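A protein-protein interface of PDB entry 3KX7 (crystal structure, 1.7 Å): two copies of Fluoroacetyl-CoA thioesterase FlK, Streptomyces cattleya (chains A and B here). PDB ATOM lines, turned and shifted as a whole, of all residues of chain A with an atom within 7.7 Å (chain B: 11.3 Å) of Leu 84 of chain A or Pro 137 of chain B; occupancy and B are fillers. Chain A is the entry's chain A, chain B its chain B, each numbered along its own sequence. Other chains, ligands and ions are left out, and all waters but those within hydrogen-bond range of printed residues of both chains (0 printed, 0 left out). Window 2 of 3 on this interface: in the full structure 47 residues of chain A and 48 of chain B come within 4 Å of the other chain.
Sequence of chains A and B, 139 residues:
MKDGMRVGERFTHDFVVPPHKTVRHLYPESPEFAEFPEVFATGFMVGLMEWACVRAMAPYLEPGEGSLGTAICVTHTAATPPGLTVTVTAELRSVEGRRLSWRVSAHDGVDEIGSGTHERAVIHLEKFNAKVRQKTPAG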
ATOM      1  N   PHE A  15       8.694  -5.166 -22.806  1.00  0.00           N
ATOM      2  CA  PHE A  15       9.774  -4.251 -23.187  1.00  0.00           C
ATOM      3  C   PHE A  15      10.622  -4.876 -24.274  1.00  0.00           C
ATOM      4  O   PHE A  15      11.284  -5.892 -24.061  1.00  0.00           O
ATOM      5  CB  PHE A  15      10.637  -3.926 -21.960  1.00  0.00           C
ATOM      6  CG  PHE A  15      11.778  -2.985 -22.225  1.00  0.00           C
ATOM      7  CD1 PHE A  15      11.549  -1.628 -22.443  1.00  0.00           C
ATOM      8  CD2 PHE A  15      13.099  -3.458 -22.227  1.00  0.00           C
ATOM      9  CE1 PHE A  15      12.608  -0.747 -22.668  1.00  0.00           C
ATOM     10  CE2 PHE A  15      14.173  -2.579 -22.467  1.00  0.00           C
ATOM     11  CZ  PHE A  15      13.926  -1.228 -22.678  1.00  0.00           C
ATOM     12  N   VAL A  16      10.607  -4.254 -25.453  1.00  0.00           N
ATOM     13  CA  VAL A  16      11.448  -4.697 -26.545  1.00  0.00           C
ATOM     14  C   VAL A  16      12.861  -4.217 -26.231  1.00  0.00           C
ATOM     15  O   VAL A  16      13.068  -3.024 -25.975  1.00  0.00           O
ATOM     16  CB  VAL A  16      10.961  -4.147 -27.895  1.00  0.00           C
ATOM     17  CG1 VAL A  16      11.995  -4.441 -28.968  1.00  0.00           C
ATOM     18  CG2 VAL A  16       9.594  -4.777 -28.260  1.00  0.00           C
ATOM     19  N   VAL A  17      13.805  -5.156 -26.172  1.00  0.00           N
ATOM     20  CA  VAL A  17      15.198  -4.812 -25.824  1.00  0.00           C
ATOM     21  C   VAL A  17      15.866  -4.063 -26.967  1.00  0.00           C
ATOM     22  O   VAL A  17      16.010  -4.601 -28.067  1.00  0.00           O
ATOM     23  CB  VAL A  17      16.033  -6.062 -25.448  1.00  0.00           C
ATOM     24  CG1 VAL A  17      17.471  -5.639 -25.102  1.00  0.00           C
ATOM     25  CG2 VAL A  17      15.372  -6.825 -24.292  1.00  0.00           C
ATOM     26  N   PRO A  18      16.268  -2.802 -26.722  1.00  0.00           N
ATOM     27  CA  PRO A  18      16.997  -2.054 -27.734  1.00  0.00           C
ATOM     28  C   PRO A  18      18.499  -2.305 -27.625  1.00  0.00           C
ATOM     29  O   PRO A  18      18.961  -2.825 -26.597  1.00  0.00           O
ATOM     30  CB  PRO A  18      16.685  -0.608 -27.366  1.00  0.00           C
ATOM     31  CG  PRO A  18      16.614  -0.627 -25.889  1.00  0.00           C
ATOM     32  CD  PRO A  18      16.021  -1.985 -25.525  1.00  0.00           C
ATOM     33  N   ALA A  79      20.130 -15.771 -22.212  1.00  0.00           N
ATOM     34  CA  ALA A  79      20.628 -14.502 -22.752  1.00  0.00           C
ATOM     35  C   ALA A  79      19.690 -13.927 -23.804  1.00  0.00           C
ATOM     36  O   ALA A  79      19.112 -14.650 -24.599  1.00  0.00           O
ATOM     37  CB  ALA A  79      22.019 -14.701 -23.375  1.00  0.00           C
ATOM     38  N   THR A  80      19.588 -12.617 -23.829  1.00  0.00           N
ATOM     39  CA  THR A  80      18.601 -11.973 -24.710  1.00  0.00           C
ATOM     40  C   THR A  80      19.284 -10.925 -25.575  1.00  0.00           C
ATOM     41  O   THR A  80      19.733  -9.894 -25.067  1.00  0.00           O
ATOM     42  CB  THR A  80      17.495 -11.290 -23.850  1.00  0.00           C
ATOM     43  OG1 THR A  80      16.876 -12.267 -22.982  1.00  0.00           O
ATOM     44  CG2 THR A  80      16.450 -10.643 -24.741  1.00  0.00           C
ATOM     45  N   PRO A  81      19.345 -11.165 -26.905  1.00  0.00           N
ATOM     46  CA  PRO A  81      19.864 -10.145 -27.819  1.00  0.00           C
ATOM     47  C   PRO A  81      18.844  -9.025 -28.042  1.00  0.00           C
ATOM     48  O   PRO A  81      17.640  -9.226 -27.820  1.00  0.00           O
ATOM     49  CB  PRO A  81      20.092 -10.927 -29.121  1.00  0.00           C
ATOM     50  CG  PRO A  81      19.092 -12.014 -29.080  1.00  0.00           C
ATOM     51  CD  PRO A  81      18.943 -12.394 -27.617  1.00  0.00           C
ATOM     52  N   PRO A  82      19.304  -7.846 -28.479  1.00  0.00           N
ATOM     53  CA  PRO A  82      18.363  -6.793 -28.841  1.00  0.00           C
ATOM     54  C   PRO A  82      17.311  -7.268 -29.844  1.00  0.00           C
ATOM     55  O   PRO A  82      17.605  -8.098 -30.715  1.00  0.00           O
ATOM     56  CB  PRO A  82      19.270  -5.718 -29.456  1.00  0.00           C
ATOM     57  CG  PRO A  82      20.567  -5.904 -28.674  1.00  0.00           C
ATOM     58  CD  PRO A  82      20.702  -7.399 -28.639  1.00  0.00           C
ATOM     59  N   GLY A  83      16.088  -6.785 -29.686  1.00  0.00           N
ATOM     60  CA  GLY A  83      15.016  -7.125 -30.643  1.00  0.00           C
ATOM     61  C   GLY A  83      13.898  -7.984 -30.082  1.00  0.00           C
ATOM     62  O   GLY A  83      12.747  -7.858 -30.510  1.00  0.00           O
ATOM     63  N   LEU A  84      14.233  -8.867 -29.139  1.00  0.00           N
ATOM     64  CA  LEU A  84      13.246  -9.697 -28.457  1.00  0.00           C
ATOM     65  C   LEU A  84      12.470  -8.896 -27.422  1.00  0.00           C
ATOM     66  O   LEU A  84      12.966  -7.891 -26.895  1.00  0.00           O
ATOM     67  CB  LEU A  84      13.914 -10.922 -27.794  1.00  0.00           C
ATOM     68  CG  LEU A  84      14.478 -12.067 -28.654  1.00  0.00           C
ATOM     69  CD1 LEU A  84      14.925 -13.255 -27.790  1.00  0.00           C
ATOM     70  CD2 LEU A  84      13.488 -12.554 -29.703  1.00  0.00           C
ATOM     71  N   THR A  85      11.260  -9.349 -27.101  1.00  0.00           N
ATOM     72  CA  THR A  85      10.446  -8.700 -26.098  1.00  0.00           C
ATOM     73  C   THR A  85      10.632  -9.415 -24.762  1.00  0.00           C
ATOM     74  O   THR A  85      10.348 -10.619 -24.667  1.00  0.00           O
ATOM     75  CB  THR A  85       8.960  -8.778 -26.455  1.00  0.00           C
ATOM     76  OG1 THR A  85       8.778  -8.168 -27.737  1.00  0.00           O
ATOM     77  CG2 THR A  85       8.103  -8.049 -25.431  1.00  0.00           C
ATOM     78  N   VAL A  86      11.129  -8.680 -23.774  1.00  0.00           N
ATOM     79  CA  VAL A  86      11.139  -9.162 -22.389  1.00  0.00           C
ATOM     80  C   VAL A  86       9.832  -8.811 -21.681  1.00  0.00           C
ATOM     81  O   VAL A  86       9.495  -7.621 -21.511  1.00  0.00           O
ATOM     82  CB  VAL A  86      12.338  -8.644 -21.570  1.00  0.00           C
ATOM     83  CG1 VAL A  86      12.271  -9.179 -20.136  1.00  0.00           C
ATOM     84  CG2 VAL A  86      13.666  -9.094 -22.230  1.00  0.00           C
ATOM     85  N   THR A  87       9.122  -9.852 -21.257  1.00  0.00           N
ATOM     86  CA  THR A  87       7.917  -9.699 -20.444  1.00  0.00           C
ATOM     87  C   THR A  87       8.280 -10.035 -18.995  1.00  0.00           C
ATOM     88  O   THR A  87       8.713 -11.154 -18.708  1.00  0.00           O
ATOM     89  CB  THR A  87       6.788 -10.629 -20.933  1.00  0.00           C
ATOM     90  OG1 THR A  87       6.332 -10.198 -22.230  1.00  0.00           O
ATOM     91  CG2 THR A  87       5.600 -10.570 -19.962  1.00  0.00           C
ATOM     92  N   HIS A 107      10.739 -13.371 -19.225  1.00  0.00           N
ATOM     93  CA  HIS A 107      10.952 -14.299 -20.334  1.00  0.00           C
ATOM     94  C   HIS A 107      10.989 -13.459 -21.579  1.00  0.00           C
ATOM     95  O   HIS A 107      10.399 -12.375 -21.640  1.00  0.00           O
ATOM     96  CB  HIS A 107       9.843 -15.357 -20.445  1.00  0.00           C
ATOM     97  CG  HIS A 107       8.703 -14.939 -21.321  1.00  0.00           C
ATOM     98  ND1 HIS A 107       7.510 -14.464 -20.822  1.00  0.00           N
ATOM     99  CD2 HIS A 107       8.586 -14.904 -22.669  1.00  0.00           C
ATOM    100  CE1 HIS A 107       6.709 -14.150 -21.825  1.00  0.00           C
ATOM    101  NE2 HIS A 107       7.343 -14.393 -22.957  1.00  0.00           N
ATOM    102  N   ASP A 108      11.744 -13.924 -22.567  1.00  0.00           N
ATOM    103  CA  ASP A 108      12.001 -13.061 -23.712  1.00  0.00           C
ATOM    104  C   ASP A 108      11.296 -13.559 -24.974  1.00  0.00           C
ATOM    105  O   ASP A 108      11.672 -13.181 -26.073  1.00  0.00           O
ATOM    106  CB  ASP A 108      13.524 -12.889 -23.917  1.00  0.00           C
ATOM    107  CG  ASP A 108      14.223 -14.175 -24.307  1.00  0.00           C
ATOM    108  OD1 ASP A 108      13.541 -15.172 -24.637  1.00  0.00           O
ATOM    109  OD2 ASP A 108      15.471 -14.190 -24.284  1.00  0.00           O
ATOM    110  N   GLY A 109      10.287 -14.410 -24.798  1.00  0.00           N
ATOM    111  CA  GLY A 109       9.574 -15.018 -25.934  1.00  0.00           C
ATOM    112  C   GLY A 109      10.184 -16.316 -26.433  1.00  0.00           C
ATOM    113  O   GLY A 109       9.513 -17.108 -27.112  1.00  0.00           O
ATOM    114  N   VAL A 110      11.448 -16.556 -26.108  1.00  0.00           N
ATOM    115  CA  VAL A 110      12.105 -17.810 -26.479  1.00  0.00           C
ATOM    116  C   VAL A 110      12.345 -18.649 -25.225  1.00  0.00           C
ATOM    117  O   VAL A 110      12.010 -19.842 -25.179  1.00  0.00           O
ATOM    118  CB  VAL A 110      13.426 -17.541 -27.251  1.00  0.00           C
ATOM    119  CG1 VAL A 110      14.094 -18.847 -27.687  1.00  0.00           C
ATOM    120  CG2 VAL A 110      13.155 -16.638 -28.469  1.00  0.00           C
ATOM    121  N   ASP A 111      12.918 -17.999 -24.210  1.00  0.00           N
ATOM    122  CA  ASP A 111      13.323 -18.642 -22.971  1.00  0.00           C
ATOM    123  C   ASP A 111      12.841 -17.851 -21.775  1.00  0.00           C
ATOM    124  O   ASP A 111      12.745 -16.618 -21.832  1.00  0.00           O
ATOM    125  CB  ASP A 111      14.856 -18.710 -22.862  1.00  0.00           C
ATOM    126  CG  ASP A 111      15.504 -19.489 -23.989  1.00  0.00           C
ATOM    127  OD1 ASP A 111      15.101 -20.652 -24.184  1.00  0.00           O
ATOM    128  OD2 ASP A 111      16.426 -18.958 -24.652  1.00  0.00           O
ATOM    129  N   ILE A 113      14.132 -16.113 -18.770  1.00  0.00           N
ATOM    130  CA  ILE A 113      15.459 -15.536 -18.622  1.00  0.00           C
ATOM    131  C   ILE A 113      15.850 -15.294 -17.173  1.00  0.00           C
ATOM    132  O   ILE A 113      17.017 -15.092 -16.888  1.00  0.00           O
ATOM    133  CB  ILE A 113      15.654 -14.229 -19.458  1.00  0.00           C
ATOM    134  CG1 ILE A 113      14.722 -13.104 -19.001  1.00  0.00           C
ATOM    135  CG2 ILE A 113      15.484 -14.554 -20.963  1.00  0.00           C
ATOM    136  CD1 ILE A 113      15.155 -11.693 -19.492  1.00  0.00           C
ATOM    137  N   TYR B  27      16.776   3.809 -16.738  1.00  0.00           N
ATOM    138  CA  TYR B  27      15.749   3.743 -17.757  1.00  0.00           C
ATOM    139  C   TYR B  27      15.227   5.150 -18.108  1.00  0.00           C
ATOM    140  O   TYR B  27      14.247   5.623 -17.515  1.00  0.00           O
ATOM    141  CB  TYR B  27      14.620   2.787 -17.353  1.00  0.00           C
ATOM    142  CG  TYR B  27      14.923   1.333 -17.657  1.00  0.00           C
ATOM    143  CD1 TYR B  27      14.556   0.772 -18.884  1.00  0.00           C
ATOM    144  CD2 TYR B  27      15.613   0.524 -16.734  1.00  0.00           C
ATOM    145  CE1 TYR B  27      14.832  -0.551 -19.182  1.00  0.00           C
ATOM    146  CE2 TYR B  27      15.891  -0.812 -17.027  1.00  0.00           C
ATOM    147  CZ  TYR B  27      15.505  -1.341 -18.236  1.00  0.00           C
ATOM    148  OH  TYR B  27      15.793  -2.651 -18.566  1.00  0.00           O
ATOM    149  N   ASN B 129      28.241 -16.575 -28.357  1.00  0.00           N
ATOM    150  CA  ASN B 129      27.740 -15.600 -29.331  1.00  0.00           C
ATOM    151  C   ASN B 129      27.000 -16.275 -30.495  1.00  0.00           C
ATOM    152  O   ASN B 129      26.041 -15.717 -31.032  1.00  0.00           O
ATOM    153  CB  ASN B 129      28.867 -14.693 -29.828  1.00  0.00           C
ATOM    154  CG  ASN B 129      29.270 -13.648 -28.801  1.00  0.00           C
ATOM    155  OD1 ASN B 129      28.487 -13.286 -27.926  1.00  0.00           O
ATOM    156  ND2 ASN B 129      30.495 -13.147 -28.912  1.00  0.00           N
ATOM    157  N   ALA B 130      27.421 -17.491 -30.835  1.00  0.00           N
ATOM    158  CA  ALA B 130      26.738 -18.323 -31.825  1.00  0.00           C
ATOM    159  C   ALA B 130      25.340 -18.741 -31.359  1.00  0.00           C
ATOM    160  O   ALA B 130      24.386 -18.648 -32.130  1.00  0.00           O
ATOM    161  CB  ALA B 130      27.580 -19.555 -32.172  1.00  0.00           C
ATOM    162  N   LYS B 131      25.223 -19.210 -30.114  1.00  0.00           N
ATOM    163  CA  LYS B 131      23.915 -19.575 -29.547  1.00  0.00           C
ATOM    164  C   LYS B 131      22.991 -18.359 -29.465  1.00  0.00           C
ATOM    165  O   LYS B 131      21.791 -18.468 -29.723  1.00  0.00           O
ATOM    166  CB  LYS B 131      24.046 -20.255 -28.174  1.00  0.00           C
ATOM    167  CG  LYS B 131      25.041 -21.424 -28.110  1.00  0.00           C
ATOM    168  CD  LYS B 131      24.774 -22.526 -29.141  1.00  0.00           C
ATOM    169  CE  LYS B 131      26.022 -23.381 -29.389  1.00  0.00           C
ATOM    170  NZ  LYS B 131      26.409 -24.228 -28.214  1.00  0.00           N
ATOM    171  N   VAL B 132      23.552 -17.197 -29.125  1.00  0.00           N
ATOM    172  CA  VAL B 132      22.775 -15.942 -29.077  1.00  0.00           C
ATOM    173  C   VAL B 132      22.220 -15.588 -30.461  1.00  0.00           C
ATOM    174  O   VAL B 132      21.027 -15.309 -30.601  1.00  0.00           O
ATOM    175  CB  VAL B 132      23.604 -14.774 -28.523  1.00  0.00           C
ATOM    176  CG1 VAL B 132      22.892 -13.424 -28.739  1.00  0.00           C
ATOM    177  CG2 VAL B 132      23.903 -14.999 -27.050  1.00  0.00           C
ATOM    178  N   ARG B 133      23.091 -15.605 -31.468  1.00  0.00           N
ATOM    179  CA  ARG B 133      22.684 -15.345 -32.863  1.00  0.00           C
ATOM    180  C   ARG B 133      21.452 -16.157 -33.279  1.00  0.00           C
ATOM    181  O   ARG B 133      20.581 -15.640 -33.983  1.00  0.00           O
ATOM    182  CB  ARG B 133      23.851 -15.595 -33.835  1.00  0.00           C
ATOM    183  N   GLN B 134      21.377 -17.406 -32.812  1.00  0.00           N
ATOM    184  CA  GLN B 134      20.269 -18.323 -33.099  1.00  0.00           C
ATOM    185  C   GLN B 134      18.899 -17.845 -32.607  1.00  0.00           C
ATOM    186  O   GLN B 134      17.863 -18.319 -33.082  1.00  0.00           O
ATOM    187  CB  GLN B 134      20.559 -19.707 -32.510  1.00  0.00           C
ATOM    188  CG  GLN B 134      21.717 -20.455 -33.172  1.00  0.00           C
ATOM    189  CD  GLN B 134      22.106 -21.721 -32.421  1.00  0.00           C
ATOM    190  OE1 GLN B 134      21.245 -22.487 -31.975  1.00  0.00           O
ATOM    191  NE2 GLN B 134      23.410 -21.951 -32.286  1.00  0.00           N
ATOM    192  N   LYS B 135      18.896 -16.917 -31.649  1.00  0.00           N
ATOM    193  CA  LYS B 135      17.647 -16.351 -31.132  1.00  0.00           C
ATOM    194  C   LYS B 135      17.585 -14.837 -31.337  1.00  0.00           C
ATOM    195  O   LYS B 135      16.795 -14.139 -30.693  1.00  0.00           O
ATOM    196  CB  LYS B 135      17.414 -16.747 -29.661  1.00  0.00           C
ATOM    197  CG  LYS B 135      18.544 -16.384 -28.701  1.00  0.00           C
ATOM    198  CD  LYS B 135      18.260 -16.854 -27.270  1.00  0.00           C
ATOM    199  CE  LYS B 135      17.159 -16.034 -26.590  1.00  0.00           C
ATOM    200  NZ  LYS B 135      17.019 -16.351 -25.130  1.00  0.00           N
ATOM    201  N   THR B 136      18.425 -14.333 -32.240  1.00  0.00           N
ATOM    202  CA  THR B 136      18.370 -12.931 -32.629  1.00  0.00           C
ATOM    203  C   THR B 136      17.394 -12.753 -33.802  1.00  0.00           C
ATOM    204  O   THR B 136      17.492 -13.469 -34.806  1.00  0.00           O
ATOM    205  CB  THR B 136      19.772 -12.375 -32.975  1.00  0.00           C
ATOM    206  OG1 THR B 136      20.670 -12.632 -31.885  1.00  0.00           O
ATOM    207  CG2 THR B 136      19.724 -10.876 -33.201  1.00  0.00           C
ATOM    208  N   PRO B 137      16.439 -11.812 -33.670  1.00  0.00           N
ATOM    209  CA  PRO B 137      15.527 -11.538 -34.796  1.00  0.00           C
ATOM    210  C   PRO B 137      16.293 -11.106 -36.052  1.00  0.00           C
ATOM    211  O   PRO B 137      17.295 -10.402 -35.937  1.00  0.00           O
ATOM    212  CB  PRO B 137      14.668 -10.376 -34.283  1.00  0.00           C
ATOM    213  CG  PRO B 137      14.747 -10.461 -32.784  1.00  0.00           C
ATOM    214  CD  PRO B 137      16.137 -10.971 -32.492  1.00  0.00           C
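The side-chain amino group (NZ) of Lys 135 of chain B is in hydrogen-bond range of the backbone carbonyl oxygen (O) of Ala 79 of chain A (2.7 Å).
The side-chain amino group (NZ) of Lys 135 of chain B is in salt-bridge range of the side-chain carboxylate (OD2) of Asp 108 of chain A.
The side-chain carboxylate (OD2) of Asp 111 of chain A is in salt-bridge range of the side-chain amino group (NZ) of Lys 135 of chain B.
O of Phe 15 of chain A is in hydrogen-bond range of N of Val 86 of chain A (2.8 Å).
The backbone carbonyl oxygen of Val 17 of chain A lies within hydrogen-bond range of the backbone NH of Gly 83 of chain A, at 2.7 Å.
The backbone NH (N) of Val 17 of chain A is in hydrogen-bond range of the backbone carbonyl oxygen (O) of Leu 84 of chain A (3.0 Å).
OG1 of Thr 80 of chain A sits at hydrogen-bond distance from OD2 of Asp 108 of chain A, at 2.7 Å.
OD1 of Asp 108 of chain A sits at hydrogen-bond distance from N of Asp 111 of chain A (2.9 Å).
The backbone carbonyl oxygen (O) of Val 132 of chain B lies within hydrogen-bond range of the side-chain hydroxyl (OG1) of Thr 136 of chain B (3.0 Å).
Phe 15 of chain A touches Tyr 27 of chain B (CZ to CE1, 3.7 Å).
CB of Pro 81 of chain A touches CG1 of Val 132 of chain B (3.8 Å).
CG of Pro 81 of chain A touches O of Lys 135 of chain B, 3.5 Å away.
Pro 81 of chain A touches Thr 136 of chain B.
Pro 137 of chain B touches Pro 82 of chain A.
Gly 83 of chain A touches Pro 137 of chain B (C to CG, 3.8 Å).
Leu 84 of chain A touches Lys 135 of chain B.
Leu 84 of chain A touches Pro 137 of chain B.
Of the printed residues of chain B, Phe 15 of chain A touches Tyr 27 (3.7 Å).
No residue of chain B comes within 4 Å of Val 16 of chain A.
No residue of chain B comes within 4 Å of Val 17 of chain A.
Of the printed residues of chain B, Pro 81 of chain A touches Val 132 (3.8 Å), Lys 135 (3.5 Å) and Thr 136 (3.3 Å).
Pro 82 of chain A touches just one residue of chain B: Pro 137 (3.7 Å).
Printed residues of chain B within 4 Å of Leu 84 of chain A: Lys 135 (3.6 Å) and Pro 137 (3.9 Å).
No residue of chain B comes within 4 Å of Thr 85 of chain A.
Of the printed residues of chain B, Asp 108 of chain A touches Lys 135 (2.8 Å).
No residue of chain B comes within 4 Å of Gly 109 of chain A.
Of the printed residues of chain B, Asp 111 of chain A touches Lys 135 (2.7 Å).
Of the printed residues of chain A, Val 132 of chain B touches Pro 81 (3.8 Å).
Of chain A, only Pro 82 (3.7 Å), Gly 83 (3.8 Å) and Leu 84 (3.9 Å) come within 4 Å of Pro 137 of chain B.
Of the 10 printed residues of chain B, 5 touch a printed residue of chain A.
Printed residues of chain B that touch a printed residue of chain A: Tyr 27, Val 132, Lys 135, Thr 136 and Pro 137.
Hydrophobic or aromatic side chains of chain B within 4 Å of the printed part of chain A: Tyr 27, Val 132 and Pro 137.
Of the 19 printed residues of chain A, 8 touch a printed residue of chain B.
Hydrophobic or aromatic side chains of chain A that line the printed part of chain B: Phe 15, Pro 81 and Leu 84.
Along chain A the printed residues that touch a printed residue of chain B span positions 15 to 111.
Among the printed residues, Asp or Glu carboxylates within 4 Å of a Lys or Arg side-chain nitrogen of the other chain: Asp 108 of chain A with Lys 135 of chain B (2.8 Å) and Asp 111 of chain A with Lys 135 of chain B (2.7 Å).
No position is printed for both chains.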
